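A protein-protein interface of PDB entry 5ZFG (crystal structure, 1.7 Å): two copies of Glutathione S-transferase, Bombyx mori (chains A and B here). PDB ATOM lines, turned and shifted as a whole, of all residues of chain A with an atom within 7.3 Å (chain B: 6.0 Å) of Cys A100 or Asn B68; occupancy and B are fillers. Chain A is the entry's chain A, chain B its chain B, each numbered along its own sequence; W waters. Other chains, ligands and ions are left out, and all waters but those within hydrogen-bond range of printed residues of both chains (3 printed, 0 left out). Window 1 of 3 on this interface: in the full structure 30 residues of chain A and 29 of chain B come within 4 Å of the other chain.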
ATOM      1  N   ASN A  68     -15.928  -6.631 -23.969  1.00  0.00           N
ATOM      2  CA  ASN A  68     -16.597  -6.622 -25.273  1.00  0.00           C
ATOM      3  C   ASN A  68     -15.793  -5.823 -26.298  1.00  0.00           C
ATOM      4  O   ASN A  68     -15.638  -6.251 -27.450  1.00  0.00           O
ATOM      5  CB  ASN A  68     -18.004  -6.045 -25.168  1.00  0.00           C
ATOM      6  CG  ASN A  68     -18.994  -6.996 -24.532  1.00  0.00           C
ATOM      7  OD1 ASN A  68     -18.669  -8.125 -24.171  1.00  0.00           O
ATOM      8  ND2 ASN A  68     -20.220  -6.517 -24.359  1.00  0.00           N
ATOM      9  N   GLN A  72     -13.931  -7.145 -29.806  1.00  0.00           N
ATOM     10  CA  GLN A  72     -14.089  -6.509 -31.114  1.00  0.00           C
ATOM     11  C   GLN A  72     -12.740  -6.072 -31.692  1.00  0.00           C
ATOM     12  O   GLN A  72     -12.491  -6.223 -32.899  1.00  0.00           O
ATOM     13  CB  GLN A  72     -15.055  -5.329 -30.979  1.00  0.00           C
ATOM     14  CG  GLN A  72     -16.484  -5.807 -30.656  1.00  0.00           C
ATOM     15  CD  GLN A  72     -17.378  -4.737 -30.052  1.00  0.00           C
ATOM     16  OE1 GLN A  72     -16.915  -3.840 -29.348  1.00  0.00           O
ATOM     17  NE2 GLN A  72     -18.682  -4.849 -30.303  1.00  0.00           N
ATOM     18  N   ILE A  94     -25.941  -8.410 -35.300  1.00  0.00           N
ATOM     19  CA  ILE A  94     -26.412  -9.487 -34.431  1.00  0.00           C
ATOM     20  C   ILE A  94     -25.340  -9.843 -33.405  1.00  0.00           C
ATOM     21  O   ILE A  94     -25.639 -10.042 -32.221  1.00  0.00           O
ATOM     22  CB  ILE A  94     -26.852 -10.720 -35.246  1.00  0.00           C
ATOM     23  CG1 ILE A  94     -27.945 -10.328 -36.252  1.00  0.00           C
ATOM     24  CG2 ILE A  94     -27.396 -11.813 -34.285  1.00  0.00           C
ATOM     25  CD1 ILE A  94     -28.257 -11.407 -37.287  1.00  0.00           C
ATOM     26  N   VAL A  95     -24.073  -9.897 -33.836  1.00  0.00           N
ATOM     27  CA  VAL A  95     -22.978 -10.132 -32.894  1.00  0.00           C
ATOM     28  C   VAL A  95     -22.916  -9.024 -31.856  1.00  0.00           C
ATOM     29  O   VAL A  95     -22.877  -9.289 -30.647  1.00  0.00           O
ATOM     30  CB  VAL A  95     -21.636 -10.270 -33.633  1.00  0.00           C
ATOM     31  CG1 VAL A  95     -20.474 -10.312 -32.597  1.00  0.00           C
ATOM     32  CG2 VAL A  95     -21.662 -11.536 -34.486  1.00  0.00           C
ATOM     33  N   ASN A  96     -22.909  -7.767 -32.316  1.00  0.00           N
ATOM     34  CA  ASN A  96     -22.843  -6.628 -31.409  1.00  0.00           C
ATOM     35  C   ASN A  96     -23.999  -6.635 -30.427  1.00  0.00           C
ATOM     36  O   ASN A  96     -23.806  -6.354 -29.238  1.00  0.00           O
ATOM     37  CB  ASN A  96     -22.832  -5.323 -32.196  1.00  0.00           C
ATOM     38  CG  ASN A  96     -21.495  -5.063 -32.894  1.00  0.00           C
ATOM     39  OD1 ASN A  96     -20.477  -5.713 -32.609  1.00  0.00           O
ATOM     40  ND2 ASN A  96     -21.497  -4.104 -33.822  1.00  0.00           N
ATOM     41  N   HIS A  97     -25.205  -6.954 -30.904  1.00  0.00           N
ATOM     42  CA  HIS A  97     -26.347  -7.027 -30.005  1.00  0.00           C
ATOM     43  C   HIS A  97     -26.118  -8.060 -28.909  1.00  0.00           C
ATOM     44  O   HIS A  97     -26.335  -7.792 -27.717  1.00  0.00           O
ATOM     45  CB  HIS A  97     -27.627  -7.386 -30.758  1.00  0.00           C
ATOM     46  CG  HIS A  97     -28.742  -7.671 -29.811  1.00  0.00           C
ATOM     47  ND1 HIS A  97     -28.954  -8.924 -29.278  1.00  0.00           N
ATOM     48  CD2 HIS A  97     -29.591  -6.836 -29.165  1.00  0.00           C
ATOM     49  CE1 HIS A  97     -29.931  -8.861 -28.390  1.00  0.00           C
ATOM     50  NE2 HIS A  97     -30.335  -7.606 -28.303  1.00  0.00           N
ATOM     51  N   ARG A  98     -25.696  -9.268 -29.303  1.00  0.00           N
ATOM     52  CA  ARG A  98     -25.529 -10.335 -28.325  1.00  0.00           C
ATOM     53  C   ARG A  98     -24.462  -9.990 -27.289  1.00  0.00           C
ATOM     54  O   ARG A  98     -24.598 -10.365 -26.115  1.00  0.00           O
ATOM     55  CB  ARG A  98     -25.200 -11.657 -29.038  1.00  0.00           C
ATOM     56  CG  ARG A  98     -26.306 -12.195 -29.989  1.00  0.00           C
ATOM     57  CD  ARG A  98     -27.629 -12.507 -29.293  1.00  0.00           C
ATOM     58  NE  ARG A  98     -28.553 -13.144 -30.243  1.00  0.00           N
ATOM     59  CZ  ARG A  98     -29.395 -12.494 -31.044  1.00  0.00           C
ATOM     60  NH1 ARG A  98     -29.479 -11.166 -31.020  1.00  0.00           N
ATOM     61  NH2 ARG A  98     -30.158 -13.183 -31.881  1.00  0.00           N
ATOM     62  N   LEU A  99     -23.417  -9.257 -27.692  1.00  0.00           N
ATOM     63  CA  LEU A  99     -22.416  -8.770 -26.744  1.00  0.00           C
ATOM     64  C   LEU A  99     -23.042  -7.796 -25.747  1.00  0.00           C
ATOM     65  O   LEU A  99     -22.864  -7.934 -24.534  1.00  0.00           O
ATOM     66  CB  LEU A  99     -21.258  -8.098 -27.498  1.00  0.00           C
ATOM     67  CG  LEU A  99     -20.323  -9.016 -28.318  1.00  0.00           C
ATOM     68  CD1 LEU A  99     -19.330  -8.202 -29.169  1.00  0.00           C
ATOM     69  CD2 LEU A  99     -19.575  -9.999 -27.377  1.00  0.00           C
ATOM     70  N   CYS A 100     -23.803  -6.818 -26.253  1.00  0.00           N
ATOM     71  CA  CYS A 100     -24.480  -5.871 -25.370  1.00  0.00           C
ATOM     72  C   CYS A 100     -25.467  -6.578 -24.447  1.00  0.00           C
ATOM     73  O   CYS A 100     -25.564  -6.245 -23.261  1.00  0.00           O
ATOM     74  CB  CYS A 100     -25.218  -4.813 -26.199  1.00  0.00           C
ATOM     75  SG  CYS A 100     -24.148  -3.682 -27.093  1.00  0.00           S
ATOM     76  N   PHE A 101     -26.232  -7.533 -24.994  1.00  0.00           N
ATOM     77  CA  PHE A 101     -27.215  -8.284 -24.209  1.00  0.00           C
ATOM     78  C   PHE A 101     -26.544  -9.040 -23.066  1.00  0.00           C
ATOM     79  O   PHE A 101     -27.062  -9.077 -21.945  1.00  0.00           O
ATOM     80  CB  PHE A 101     -27.975  -9.247 -25.137  1.00  0.00           C
ATOM     81  CG  PHE A 101     -28.793 -10.309 -24.413  1.00  0.00           C
ATOM     82  CD1 PHE A 101     -29.841  -9.954 -23.580  1.00  0.00           C
ATOM     83  CD2 PHE A 101     -28.516 -11.662 -24.598  1.00  0.00           C
ATOM     84  CE1 PHE A 101     -30.597 -10.921 -22.927  1.00  0.00           C
ATOM     85  CE2 PHE A 101     -29.264 -12.644 -23.939  1.00  0.00           C
ATOM     86  CZ  PHE A 101     -30.309 -12.267 -23.110  1.00  0.00           C
ATOM     87  N   ASN A 102     -25.376  -9.632 -23.317  1.00  0.00           N
ATOM     88  CA  ASN A 102     -24.679 -10.288 -22.213  1.00  0.00           C
ATOM     89  C   ASN A 102     -24.291  -9.290 -21.132  1.00  0.00           C
ATOM     90  O   ASN A 102     -24.488  -9.543 -19.935  1.00  0.00           O
ATOM     91  CB  ASN A 102     -23.432 -11.022 -22.707  1.00  0.00           C
ATOM     92  CG  ASN A 102     -22.807 -11.815 -21.601  1.00  0.00           C
ATOM     93  OD1 ASN A 102     -23.372 -12.823 -21.182  1.00  0.00           O
ATOM     94  ND2 ASN A 102     -21.679 -11.342 -21.071  1.00  0.00           N
ATOM     95  N   LEU A 103     -23.758  -8.140 -21.538  1.00  0.00           N
ATOM     96  CA  LEU A 103     -23.260  -7.156 -20.582  1.00  0.00           C
ATOM     97  C   LEU A 103     -24.403  -6.499 -19.813  1.00  0.00           C
ATOM     98  O   LEU A 103     -24.317  -6.325 -18.588  1.00  0.00           O
ATOM     99  CB  LEU A 103     -22.434  -6.096 -21.323  1.00  0.00           C
ATOM    100  CG  LEU A 103     -21.983  -4.819 -20.587  1.00  0.00           C
ATOM    101  CD1 LEU A 103     -21.193  -5.153 -19.341  1.00  0.00           C
ATOM    102  CD2 LEU A 103     -21.132  -3.915 -21.498  1.00  0.00           C
ATOM    103  N   SER A 104     -25.475  -6.139 -20.515  1.00  0.00           N
ATOM    104  CA  SER A 104     -26.553  -5.370 -19.899  1.00  0.00           C
ATOM    105  C   SER A 104     -27.513  -6.224 -19.079  1.00  0.00           C
ATOM    106  O   SER A 104     -28.152  -5.701 -18.152  1.00  0.00           O
ATOM    107  CB  SER A 104     -27.368  -4.651 -20.975  1.00  0.00           C
ATOM    108  OG  SER A 104     -28.187  -5.567 -21.693  1.00  0.00           O
ATOM    109  N   SER A 105     -27.635  -7.515 -19.399  1.00  0.00           N
ATOM    110  CA  SER A 105     -28.785  -8.299 -18.960  1.00  0.00           C
ATOM    111  C   SER A 105     -28.439  -9.732 -18.565  1.00  0.00           C
ATOM    112  O   SER A 105     -28.664 -10.136 -17.417  1.00  0.00           O
ATOM    113  CB  SER A 105     -29.849  -8.317 -20.069  1.00  0.00           C
ATOM    114  OG  SER A 105     -30.215  -7.000 -20.450  1.00  0.00           O
ATOM    115  N   TYR A 106     -27.931 -10.524 -19.509  1.00  0.00           N
ATOM    116  CA  TYR A 106     -27.768 -11.956 -19.266  1.00  0.00           C
ATOM    117  C   TYR A 106     -26.749 -12.211 -18.163  1.00  0.00           C
ATOM    118  O   TYR A 106     -27.059 -12.844 -17.149  1.00  0.00           O
ATOM    119  CB  TYR A 106     -27.361 -12.658 -20.560  1.00  0.00           C
ATOM    120  CG  TYR A 106     -27.447 -14.173 -20.578  1.00  0.00           C
ATOM    121  CD1 TYR A 106     -28.671 -14.826 -20.758  1.00  0.00           C
ATOM    122  CD2 TYR A 106     -26.296 -14.957 -20.473  1.00  0.00           C
ATOM    123  CE1 TYR A 106     -28.746 -16.216 -20.815  1.00  0.00           C
ATOM    124  CE2 TYR A 106     -26.359 -16.356 -20.536  1.00  0.00           C
ATOM    125  CZ  TYR A 106     -27.589 -16.980 -20.697  1.00  0.00           C
ATOM    126  OH  TYR A 106     -27.644 -18.366 -20.750  1.00  0.00           O
ATOM    127  N   VAL B  17     -29.641   7.423 -30.106  1.00  0.00           N
ATOM    128  CA  VAL B  17     -29.891   6.855 -31.424  1.00  0.00           C
ATOM    129  C   VAL B  17     -30.476   7.923 -32.346  1.00  0.00           C
ATOM    130  O   VAL B  17     -30.091   8.029 -33.515  1.00  0.00           O
ATOM    131  CB  VAL B  17     -30.801   5.617 -31.337  1.00  0.00           C
ATOM    132  CG1 VAL B  17     -31.195   5.132 -32.741  1.00  0.00           C
ATOM    133  CG2 VAL B  17     -30.105   4.455 -30.580  1.00  0.00           C
ATOM    134  N   GLU B  66     -30.799  -2.855 -28.100  1.00  0.00           N
ATOM    135  CA  GLU B  66     -29.545  -2.376 -27.513  1.00  0.00           C
ATOM    136  C   GLU B  66     -29.020  -1.141 -28.244  1.00  0.00           C
ATOM    137  O   GLU B  66     -28.477  -1.246 -29.353  1.00  0.00           O
ATOM    138  CB  GLU B  66     -28.480  -3.487 -27.485  1.00  0.00           C
ATOM    139  CG  GLU B  66     -28.853  -4.629 -26.546  1.00  0.00           C
ATOM    140  CD  GLU B  66     -28.615  -4.317 -25.077  1.00  0.00           C
ATOM    141  OE1 GLU B  66     -28.039  -3.259 -24.747  1.00  0.00           O
ATOM    142  OE2 GLU B  66     -29.002  -5.152 -24.221  1.00  0.00           O
ATOM    143  N   SER B  67     -29.151   0.029 -27.602  1.00  0.00           N
ATOM    144  CA  SER B  67     -28.850   1.296 -28.278  1.00  0.00           C
ATOM    145  C   SER B  67     -27.402   1.366 -28.785  1.00  0.00           C
ATOM    146  O   SER B  67     -27.150   1.925 -29.865  1.00  0.00           O
ATOM    147  CB  SER B  67     -29.168   2.482 -27.353  1.00  0.00           C
ATOM    148  OG  SER B  67     -28.374   2.511 -26.181  1.00  0.00           O
ATOM    149  N   ASN B  68     -26.433   0.789 -28.045  1.00  0.00           N
ATOM    150  CA  ASN B  68     -25.051   0.779 -28.534  1.00  0.00           C
ATOM    151  C   ASN B  68     -24.937   0.011 -29.847  1.00  0.00           C
ATOM    152  O   ASN B  68     -24.286   0.468 -30.792  1.00  0.00           O
ATOM    153  CB  ASN B  68     -24.115   0.167 -27.500  1.00  0.00           C
ATOM    154  CG  ASN B  68     -23.832   1.093 -26.355  1.00  0.00           C
ATOM    155  OD1 ASN B  68     -24.296   2.231 -26.329  1.00  0.00           O
ATOM    156  ND2 ASN B  68     -23.087   0.600 -25.370  1.00  0.00           N
ATOM    157  N   ALA B  69     -25.562  -1.160 -29.918  1.00  0.00           N
ATOM    158  CA  ALA B  69     -25.535  -1.942 -31.154  1.00  0.00           C
ATOM    159  C   ALA B  69     -26.284  -1.232 -32.278  1.00  0.00           C
ATOM    160  O   ALA B  69     -25.889  -1.322 -33.449  1.00  0.00           O
ATOM    161  CB  ALA B  69     -26.140  -3.318 -30.899  1.00  0.00           C
ATOM    162  N   ILE B  70     -27.381  -0.539 -31.942  1.00  0.00           N
ATOM    163  CA  ILE B  70     -28.098   0.239 -32.959  1.00  0.00           C
ATOM    164  C   ILE B  70     -27.202   1.341 -33.510  1.00  0.00           C
ATOM    165  O   ILE B  70     -27.127   1.543 -34.731  1.00  0.00           O
ATOM    166  CB  ILE B  70     -29.405   0.822 -32.390  1.00  0.00           C
ATOM    167  CG1 ILE B  70     -30.374  -0.297 -31.979  1.00  0.00           C
ATOM    168  CG2 ILE B  70     -30.074   1.747 -33.450  1.00  0.00           C
ATOM    169  CD1 ILE B  70     -31.579   0.220 -31.178  1.00  0.00           C
ATOM    170  N   LEU B  71     -26.480   2.048 -32.625  1.00  0.00           N
ATOM    171  CA  LEU B  71     -25.552   3.088 -33.068  1.00  0.00           C
ATOM    172  C   LEU B  71     -24.503   2.523 -34.025  1.00  0.00           C
ATOM    173  O   LEU B  71     -24.213   3.108 -35.084  1.00  0.00           O
ATOM    174  CB  LEU B  71     -24.868   3.740 -31.864  1.00  0.00           C
ATOM    175  CG  LEU B  71     -25.736   4.599 -30.928  1.00  0.00           C
ATOM    176  CD1 LEU B  71     -24.960   5.029 -29.703  1.00  0.00           C
ATOM    177  CD2 LEU B  71     -26.244   5.813 -31.697  1.00  0.00           C
ATOM    178  N   GLN B  72     -23.920   1.385 -33.669  1.00  0.00           N
ATOM    179  CA  GLN B  72     -22.904   0.771 -34.526  1.00  0.00           C
ATOM    180  C   GLN B  72     -23.488   0.346 -35.873  1.00  0.00           C
ATOM    181  O   GLN B  72     -22.852   0.523 -36.926  1.00  0.00           O
ATOM    182  CB  GLN B  72     -22.279  -0.412 -33.782  1.00  0.00           C
ATOM    183  CG  GLN B  72     -21.479   0.065 -32.556  1.00  0.00           C
ATOM    184  CD  GLN B  72     -21.239  -1.017 -31.518  1.00  0.00           C
ATOM    185  OE1 GLN B  72     -22.053  -1.919 -31.349  1.00  0.00           O
ATOM    186  NE2 GLN B  72     -20.112  -0.914 -30.803  1.00  0.00           N
ATOM    187  N   TYR B  73     -24.717  -0.170 -35.861  1.00  0.00           N
ATOM    188  CA  TYR B  73     -25.328  -0.694 -37.081  1.00  0.00           C
ATOM    189  C   TYR B  73     -25.675   0.425 -38.052  1.00  0.00           C
ATOM    190  O   TYR B  73     -25.419   0.306 -39.252  1.00  0.00           O
ATOM    191  CB  TYR B  73     -26.574  -1.496 -36.723  1.00  0.00           C
ATOM    192  CG  TYR B  73     -27.470  -1.832 -37.910  1.00  0.00           C
ATOM    193  CD1 TYR B  73     -27.070  -2.768 -38.849  1.00  0.00           C
ATOM    194  CD2 TYR B  73     -28.694  -1.209 -38.075  1.00  0.00           C
ATOM    195  CE1 TYR B  73     -27.875  -3.085 -39.930  1.00  0.00           C
ATOM    196  CE2 TYR B  73     -29.510  -1.509 -39.164  1.00  0.00           C
ATOM    197  CZ  TYR B  73     -29.087  -2.454 -40.081  1.00  0.00           C
ATOM    198  OH  TYR B  73     -29.889  -2.784 -41.155  1.00  0.00           O
ATOM    199  N   LEU B  99     -18.413   3.395 -25.617  1.00  0.00           N
ATOM    200  CA  LEU B  99     -19.789   2.906 -25.612  1.00  0.00           C
ATOM    201  C   LEU B  99     -20.008   1.914 -24.469  1.00  0.00           C
ATOM    202  O   LEU B  99     -20.988   2.011 -23.726  1.00  0.00           O
ATOM    203  CB  LEU B  99     -20.115   2.247 -26.957  1.00  0.00           C
ATOM    204  CG  LEU B  99     -20.275   3.187 -28.165  1.00  0.00           C
ATOM    205  CD1 LEU B  99     -20.441   2.391 -29.471  1.00  0.00           C
ATOM    206  CD2 LEU B  99     -21.478   4.160 -27.973  1.00  0.00           C
ATOM    207  N   CYS B 100     -19.088   0.956 -24.319  1.00  0.00           N
ATOM    208  CA  CYS B 100     -19.192  -0.016 -23.234  1.00  0.00           C
ATOM    209  C   CYS B 100     -19.114   0.662 -21.871  1.00  0.00           C
ATOM    210  O   CYS B 100     -19.857   0.307 -20.949  1.00  0.00           O
ATOM    211  CB  CYS B 100     -18.075  -1.061 -23.357  1.00  0.00           C
ATOM    212  SG  CYS B 100     -18.266  -2.196 -24.750  1.00  0.00           S
ATOM    213  N   ASN B 102     -19.963   3.707 -21.053  1.00  0.00           N
ATOM    214  CA  ASN B 102     -21.231   4.346 -20.710  1.00  0.00           C
ATOM    215  C   ASN B 102     -22.251   3.330 -20.223  1.00  0.00           C
ATOM    216  O   ASN B 102     -22.941   3.559 -19.222  1.00  0.00           O
ATOM    217  CB  ASN B 102     -21.807   5.119 -21.898  1.00  0.00           C
ATOM    218  CG  ASN B 102     -23.026   5.907 -21.489  1.00  0.00           C
ATOM    219  OD1 ASN B 102     -22.898   6.911 -20.798  1.00  0.00           O
ATOM    220  ND2 ASN B 102     -24.217   5.443 -21.879  1.00  0.00           N
ATOM    221  N   LEU B 103     -22.366   2.204 -20.920  1.00  0.00           N
ATOM    222  CA  LEU B 103     -23.363   1.196 -20.574  1.00  0.00           C
ATOM    223  C   LEU B 103     -23.044   0.531 -19.242  1.00  0.00           C
ATOM    224  O   LEU B 103     -23.942   0.327 -18.411  1.00  0.00           O
ATOM    225  CB  LEU B 103     -23.436   0.141 -21.683  1.00  0.00           C
ATOM    226  CG  LEU B 103     -24.295  -1.118 -21.454  1.00  0.00           C
ATOM    227  CD1 LEU B 103     -25.748  -0.768 -21.157  1.00  0.00           C
ATOM    228  CD2 LEU B 103     -24.236  -2.039 -22.664  1.00  0.00           C
ATOM    229  N   ILE B 158     -19.921   8.385 -32.496  1.00  0.00           N
ATOM    230  CA  ILE B 158     -21.095   7.848 -31.804  1.00  0.00           C
ATOM    231  C   ILE B 158     -20.820   7.630 -30.318  1.00  0.00           C
ATOM    232  O   ILE B 158     -21.762   7.513 -29.539  1.00  0.00           O
ATOM    233  CB  ILE B 158     -21.626   6.533 -32.436  1.00  0.00           C
ATOM    234  CG1 ILE B 158     -20.564   5.422 -32.486  1.00  0.00           C
ATOM    235  CG2 ILE B 158     -22.279   6.784 -33.821  1.00  0.00           C
ATOM    236  CD1 ILE B 158     -21.138   4.070 -32.969  1.00  0.00           C
ATOM    237  N   PRO B 162     -24.032   8.816 -26.133  1.00  0.00           N
ATOM    238  CA  PRO B 162     -24.459   8.254 -24.845  1.00  0.00           C
ATOM    239  C   PRO B 162     -23.847   8.989 -23.670  1.00  0.00           C
ATOM    240  O   PRO B 162     -24.543   9.216 -22.669  1.00  0.00           O
ATOM    241  CB  PRO B 162     -24.008   6.778 -24.937  1.00  0.00           C
ATOM    242  CG  PRO B 162     -23.947   6.510 -26.437  1.00  0.00           C
ATOM    243  CD  PRO B 162     -23.407   7.793 -26.987  1.00  0.00           C
HETATM  244  O   HOH W   1     -18.815  -2.261 -28.148  1.00  0.00           O
HETATM  245  O   HOH W   2     -21.427  -3.484 -29.115  1.00  0.00           O
HETATM  246  O   HOH W   3     -24.196  -3.269 -34.667  1.00  0.00           O
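OE1 of Gln B72 lies within hydrogen-bond range of ND2 of Asn A96 (3.3 Å). OE2 of Glu B66 lies within hydrogen-bond range of OG of Ser A104, 2.7 Å away.
The side-chain amide oxygen (OD1) of Asn A96 lies within hydrogen-bond range of the side-chain amide nitrogen (NE2) of Gln A72 (3.0 Å). The backbone carbonyl oxygen (O) of Cys A100 is in hydrogen-bond range of the side-chain hydroxyl (OG) of Ser A104 (3.1 Å). The backbone NH (N) of Tyr A106 sits at hydrogen-bond distance from the backbone carbonyl oxygen (O) of Phe A101 (3.0 Å). OG of Ser A104 sits at hydrogen-bond distance from OG of Ser A105 (2.8 Å). OE1 of Gln B72 sits close to O of Asn B68, 3.3 Å away. ND2 of Asn B68 lies within hydrogen-bond range of O of Leu B99 (3.0 Å).
SG of Cys B100 touches CB of Asn A68, at 3.9 Å. Asn A96 touches Ala B69. CD2 of His A97 touches CG of Glu B66, 3.5 Å away. His A97 touches Ala B69. Cys A100 touches Glu B66. Cys A100 touches Asn B68. CA of Phe A101 touches OE2 of Glu B66 (3.6 Å). Leu B103 touches Leu A103 (CD2 to CD2, 3.8 Å).
Printed residues of chain B within 4 Å of Asn A96: Ala B69 and Gln B72. Cys A100 touches just these residues of chain B: Glu B66 (3.5 Å) and Asn B68 (3.9 Å). Of the printed residues of chain A, Leu B103 touches Leu A103 (3.8 Å). The nearest printed residue of chain A that does not touch Ala B69 is Cys A100 (4.04 Å).
Of the 15 printed residues of chain B, 6 touch a printed residue of chain A. Hydrophobic or aromatic side chains of chain B that line the printed part of chain A: Ala B69 and Leu B103. Along chain B the printed residues that touch a printed residue of chain A span positions 66 to 103. Printed residues of chain A that touch a printed residue of chain B: Asn A68, Asn A96, His A97, Cys A100, Phe A101, Leu A103 and Ser A104. Hydrophobic or aromatic side chains of chain A within 4 Å of the printed part of chain B: His A97 and Leu A103. Among the printed residues, 10 pairs touch across the chains. Among the printed residues, no Asp or Glu carboxylate lies within 4 Å of a Lys or Arg side-chain nitrogen of the other chain.
Asn A68 touches Cys B100, and with the chains exchanged Cys A100 touches Asn B68. Leu A103 touches its own counterpart, Leu B103. Positions printed for both chains: 68, 72, 99, 100, 102 and 103. Of the 10 pairs that touch across the chains among the printed residues, 3 have their exchanged pair printed and touching as well.
Water W1 lies within hydrogen-bond range of the side-chain amide oxygen of Gln A72 (2.7 Å), the side-chain amide nitrogen of Gln B72 (3.2 Å) and the side-chain sulfur of Cys B100 (3.4 Å). Water W2 lies within hydrogen-bond range of the side-chain amide oxygen of Gln B72 (2.8 Å), the side-chain amide nitrogen of Gln A72 (3.3 Å) and the side-chain sulfur of Cys A100 (3.4 Å). Water W3 lies within hydrogen-bond range of the backbone carbonyl oxygen (O) of Ala B69 (2.9 Å), the side-chain amide nitrogen (ND2) of Asn A96 (2.9 Å) and the backbone NH (N) of Tyr B73 (3.4 Å).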
